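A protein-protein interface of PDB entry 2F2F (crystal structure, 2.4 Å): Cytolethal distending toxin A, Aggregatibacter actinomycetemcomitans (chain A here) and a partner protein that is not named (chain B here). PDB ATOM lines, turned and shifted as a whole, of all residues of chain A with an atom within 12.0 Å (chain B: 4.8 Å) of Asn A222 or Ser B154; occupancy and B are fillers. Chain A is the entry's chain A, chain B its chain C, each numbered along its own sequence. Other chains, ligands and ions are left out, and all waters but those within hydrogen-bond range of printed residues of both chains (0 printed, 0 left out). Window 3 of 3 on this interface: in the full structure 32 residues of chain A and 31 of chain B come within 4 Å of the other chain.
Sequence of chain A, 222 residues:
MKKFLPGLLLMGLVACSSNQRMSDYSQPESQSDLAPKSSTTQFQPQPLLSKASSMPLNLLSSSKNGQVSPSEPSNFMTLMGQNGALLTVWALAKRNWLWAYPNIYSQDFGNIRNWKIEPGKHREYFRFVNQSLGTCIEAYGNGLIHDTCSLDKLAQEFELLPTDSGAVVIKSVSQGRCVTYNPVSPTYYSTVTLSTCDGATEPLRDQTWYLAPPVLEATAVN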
ATOM      1  N   PRO A  70       6.330  14.457 -28.150  1.00  0.00           N
ATOM      2  CA  PRO A  70       7.558  14.052 -27.412  1.00  0.00           C
ATOM      3  C   PRO A  70       8.077  15.147 -26.472  1.00  0.00           C
ATOM      4  O   PRO A  70       7.469  16.221 -26.357  1.00  0.00           O
ATOM      5  CB  PRO A  70       8.621  13.656 -28.430  1.00  0.00           C
ATOM      6  CG  PRO A  70       7.830  13.493 -29.733  1.00  0.00           C
ATOM      7  CD  PRO A  70       6.429  14.123 -29.586  1.00  0.00           C
ATOM      8  N   ALA A 218       4.520  18.896 -35.166  1.00  0.00           N
ATOM      9  CA  ALA A 218       4.099  19.293 -33.834  1.00  0.00           C
ATOM     10  C   ALA A 218       2.953  18.456 -33.365  1.00  0.00           C
ATOM     11  O   ALA A 218       2.091  18.096 -34.145  1.00  0.00           O
ATOM     12  CB  ALA A 218       3.698  20.752 -33.843  1.00  0.00           C
ATOM     13  N   THR A 219       2.936  18.155 -32.076  1.00  0.00           N
ATOM     14  CA  THR A 219       1.862  17.345 -31.520  1.00  0.00           C
ATOM     15  C   THR A 219       0.992  18.239 -30.646  1.00  0.00           C
ATOM     16  O   THR A 219       1.510  18.973 -29.807  1.00  0.00           O
ATOM     17  CB  THR A 219       2.430  16.192 -30.667  1.00  0.00           C
ATOM     18  OG1 THR A 219       3.366  15.435 -31.448  1.00  0.00           O
ATOM     19  CG2 THR A 219       1.312  15.274 -30.187  1.00  0.00           C
ATOM     20  N   ALA A 220      -0.317  18.208 -30.866  1.00  0.00           N
ATOM     21  CA  ALA A 220      -1.222  19.017 -30.071  1.00  0.00           C
ATOM     22  C   ALA A 220      -1.257  18.487 -28.621  1.00  0.00           C
ATOM     23  O   ALA A 220      -1.467  17.292 -28.388  1.00  0.00           O
ATOM     24  CB  ALA A 220      -2.621  18.981 -30.683  1.00  0.00           C
ATOM     25  N   VAL A 221      -1.094  19.383 -27.649  1.00  0.00           N
ATOM     26  CA  VAL A 221      -1.117  18.983 -26.245  1.00  0.00           C
ATOM     27  C   VAL A 221      -2.351  19.488 -25.487  1.00  0.00           C
ATOM     28  O   VAL A 221      -2.336  19.613 -24.266  1.00  0.00           O
ATOM     29  CB  VAL A 221       0.172  19.419 -25.503  1.00  0.00           C
ATOM     30  CG1 VAL A 221       1.338  18.595 -26.004  1.00  0.00           C
ATOM     31  CG2 VAL A 221       0.445  20.895 -25.684  1.00  0.00           C
ATOM     32  N   ASN A 222      -3.411  19.796 -26.224  1.00  0.00           N
ATOM     33  CA  ASN A 222      -4.658  20.265 -25.632  1.00  0.00           C
ATOM     34  C   ASN A 222      -5.407  19.097 -24.978  1.00  0.00           C
ATOM     35  O   ASN A 222      -6.302  19.339 -24.131  1.00  0.00           O
ATOM     36  CB  ASN A 222      -5.536  20.891 -26.718  1.00  0.00           C
ATOM     37  CG  ASN A 222      -5.834  19.926 -27.852  1.00  0.00           C
ATOM     38  OD1 ASN A 222      -4.924  19.367 -28.474  1.00  0.00           O
ATOM     39  ND2 ASN A 222      -7.109  19.722 -28.121  1.00  0.00           N
ATOM     40  OXT ASN A 222      -5.097  17.936 -25.332  1.00  0.00           O
ATOM     41  N   ASP B  81     -12.427  22.318 -27.895  1.00  0.00           N
ATOM     42  CA  ASP B  81     -11.343  21.326 -27.867  1.00  0.00           C
ATOM     43  C   ASP B  81     -10.145  21.696 -26.995  1.00  0.00           C
ATOM     44  O   ASP B  81      -9.008  21.390 -27.355  1.00  0.00           O
ATOM     45  CB  ASP B  81     -10.849  21.083 -29.303  1.00  0.00           C
ATOM     46  CG  ASP B  81     -10.079  19.792 -29.453  1.00  0.00           C
ATOM     47  OD1 ASP B  81     -10.272  18.868 -28.639  1.00  0.00           O
ATOM     48  OD2 ASP B  81      -9.277  19.698 -30.398  1.00  0.00           O
ATOM     49  N   GLY B  82     -10.391  22.355 -25.865  1.00  0.00           N
ATOM     50  CA  GLY B  82      -9.309  22.731 -24.971  1.00  0.00           C
ATOM     51  C   GLY B  82      -8.445  23.887 -25.433  1.00  0.00           C
ATOM     52  O   GLY B  82      -7.434  24.208 -24.790  1.00  0.00           O
ATOM     53  N   ILE B 118      -4.663  26.280 -30.335  1.00  0.00           N
ATOM     54  CA  ILE B 118      -4.402  24.951 -29.787  1.00  0.00           C
ATOM     55  C   ILE B 118      -2.891  24.834 -29.630  1.00  0.00           C
ATOM     56  O   ILE B 118      -2.150  24.867 -30.616  1.00  0.00           O
ATOM     57  CB  ILE B 118      -4.893  23.855 -30.747  1.00  0.00           C
ATOM     58  CG1 ILE B 118      -6.385  24.052 -31.044  1.00  0.00           C
ATOM     59  CG2 ILE B 118      -4.576  22.483 -30.177  1.00  0.00           C
ATOM     60  CD1 ILE B 118      -7.324  23.401 -30.065  1.00  0.00           C
ATOM     61  N   PRO B 119      -2.418  24.649 -28.385  1.00  0.00           N
ATOM     62  CA  PRO B 119      -0.980  24.533 -28.091  1.00  0.00           C
ATOM     63  C   PRO B 119      -0.332  23.223 -28.560  1.00  0.00           C
ATOM     64  O   PRO B 119      -1.002  22.207 -28.699  1.00  0.00           O
ATOM     65  CB  PRO B 119      -0.930  24.681 -26.575  1.00  0.00           C
ATOM     66  CG  PRO B 119      -2.230  24.124 -26.117  1.00  0.00           C
ATOM     67  CD  PRO B 119      -3.240  24.475 -27.176  1.00  0.00           C
ATOM     68  N   SER B 152     -11.177  15.942 -32.582  1.00  0.00           N
ATOM     69  CA  SER B 152     -10.192  16.457 -31.646  1.00  0.00           C
ATOM     70  C   SER B 152      -8.783  16.284 -32.183  1.00  0.00           C
ATOM     71  O   SER B 152      -8.483  15.314 -32.874  1.00  0.00           O
ATOM     72  CB  SER B 152     -10.307  15.744 -30.299  1.00  0.00           C
ATOM     73  OG  SER B 152      -9.361  16.269 -29.383  1.00  0.00           O
ATOM     74  N   VAL B 153      -7.914  17.227 -31.846  1.00  0.00           N
ATOM     75  CA  VAL B 153      -6.537  17.170 -32.292  1.00  0.00           C
ATOM     76  C   VAL B 153      -5.570  16.766 -31.175  1.00  0.00           C
ATOM     77  O   VAL B 153      -4.385  16.575 -31.430  1.00  0.00           O
ATOM     78  CB  VAL B 153      -6.095  18.524 -32.897  1.00  0.00           C
ATOM     79  CG1 VAL B 153      -6.874  18.790 -34.196  1.00  0.00           C
ATOM     80  CG2 VAL B 153      -6.306  19.643 -31.890  1.00  0.00           C
ATOM     81  N   SER B 154      -6.067  16.661 -29.942  1.00  0.00           N
ATOM     82  CA  SER B 154      -5.212  16.282 -28.809  1.00  0.00           C
ATOM     83  C   SER B 154      -4.371  15.060 -29.093  1.00  0.00           C
ATOM     84  O   SER B 154      -4.887  14.039 -29.554  1.00  0.00           O
ATOM     85  CB  SER B 154      -6.024  15.955 -27.562  1.00  0.00           C
ATOM     86  OG  SER B 154      -7.064  16.886 -27.383  1.00  0.00           O
ATOM     87  N   GLY B 155      -3.084  15.159 -28.776  1.00  0.00           N
ATOM     88  CA  GLY B 155      -2.182  14.039 -28.964  1.00  0.00           C
ATOM     89  C   GLY B 155      -1.771  13.689 -30.385  1.00  0.00           C
ATOM     90  O   GLY B 155      -0.866  12.871 -30.577  1.00  0.00           O
ATOM     91  N   ARG B 156      -2.417  14.299 -31.375  1.00  0.00           N
ATOM     92  CA  ARG B 156      -2.092  14.031 -32.771  1.00  0.00           C
ATOM     93  C   ARG B 156      -0.993  14.996 -33.179  1.00  0.00           C
ATOM     94  O   ARG B 156      -0.860  16.082 -32.597  1.00  0.00           O
ATOM     95  CB  ARG B 156      -3.330  14.193 -33.650  1.00  0.00           C
ATOM     96  CG  ARG B 156      -4.336  13.073 -33.452  1.00  0.00           C
ATOM     97  CD  ARG B 156      -5.685  13.374 -34.083  1.00  0.00           C
ATOM     98  NE  ARG B 156      -5.580  13.741 -35.493  1.00  0.00           N
ATOM     99  CZ  ARG B 156      -6.457  14.521 -36.118  1.00  0.00           C
ATOM    100  NH1 ARG B 156      -7.494  15.009 -35.447  1.00  0.00           N
ATOM    101  NH2 ARG B 156      -6.293  14.826 -37.403  1.00  0.00           N
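N of Val A221 sits at hydrogen-bond distance from O of Pro B119, 3.0 Å away.
ND2 of Asn A222 sits at hydrogen-bond distance from O of Asp B81.
OG of Ser B154 lies within hydrogen-bond range of ND2 of Asn A222.
O of Ala A220 is in hydrogen-bond range of N of Gly B155.
The backbone carbonyl oxygen of Arg B156 sits at hydrogen-bond distance from the backbone NH of Ala A220, at 2.8 Å.
Ala A218 touches Arg B156.
Gly B155 touches Thr A219 (O to CG2, 3.3 Å).
Thr A219 touches Arg B156.
Ala A220 touches Pro B119.
O of Val B153 touches CB of Ala A220 (3.1 Å).
C of Ser B154 touches O of Ala A220, 3.7 Å away.
Asn A222 touches Ile B118 (OD1 to CG2, 3.6 Å).
Val B153 touches Asn A222 (CG2 to OD1, 3.7 Å).
Of chain B, only Asp B81 (2.6 Å), Ile B118 (3.6 Å), Val B153 (3.7 Å) and Ser B154 (2.9 Å) come within 4 Å of Asn A222.
Of chain A, only Ala A220 and Asn A222 come within 4 Å of Ser B154.
Of chain A, only Asn A222 (2.6 Å) comes within 4 Å of Asp B81.
Of chain A, only Asn A222 (3.6 Å) comes within 4 Å of Ile B118.
Pro B119 touches just these residues of chain A: Ala A220 (3.5 Å) and Val A221 (3.0 Å).
No residue of chain A comes within 4 Å of Ser B152.
Of chain A, only Thr A219 and Ala A220 come within 4 Å of Gly B155.
Of the printed residues of chain B, Ala A220 touches Pro B119 (3.5 Å), Val B153 (3.1 Å), Ser B154 (3.7 Å), Gly B155 (2.7 Å) and Arg B156 (2.8 Å).
Printed residues of chain B within 4 Å of Ala A218: Arg B156.
Of the printed residues of chain B, Thr A219 touches Gly B155 (3.3 Å) and Arg B156 (3.2 Å).
The nearest residue of chain B that does not touch Asn A222 is Pro B119 (4.2 Å).
The nearest printed residue of chain B that does not touch Val A221 is Gly B155 (4.8 Å).
Of the 6 printed residues of chain A, 5 touch a printed residue of chain B.
Hydrophobic or aromatic side chains of chain A within 4 Å of the printed part of chain B: Ala A220 and Val A221.
Of the 9 printed residues of chain B, 7 touch a printed residue of chain A.
Among the printed residues, no Asp or Glu carboxylate lies within 4 Å of a Lys or Arg side-chain nitrogen of the other chain.
The side-chain hydroxyl (OG) of Ser B152 lies within hydrogen-bond range of the side-chain hydroxyl (OG) of Ser B154, 3.1 Å away.
OD1 of Asp B81 is in hydrogen-bond range of OG of Ser B152, at 2.9 Å.
The guanidinium group (NH1) of Arg B156 lies within hydrogen-bond range of the backbone carbonyl oxygen (O) of Ser B152, at 2.8 Å.
OD2 of Asp B81 is in hydrogen-bond range of N of Val B153, 3.2 Å away.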
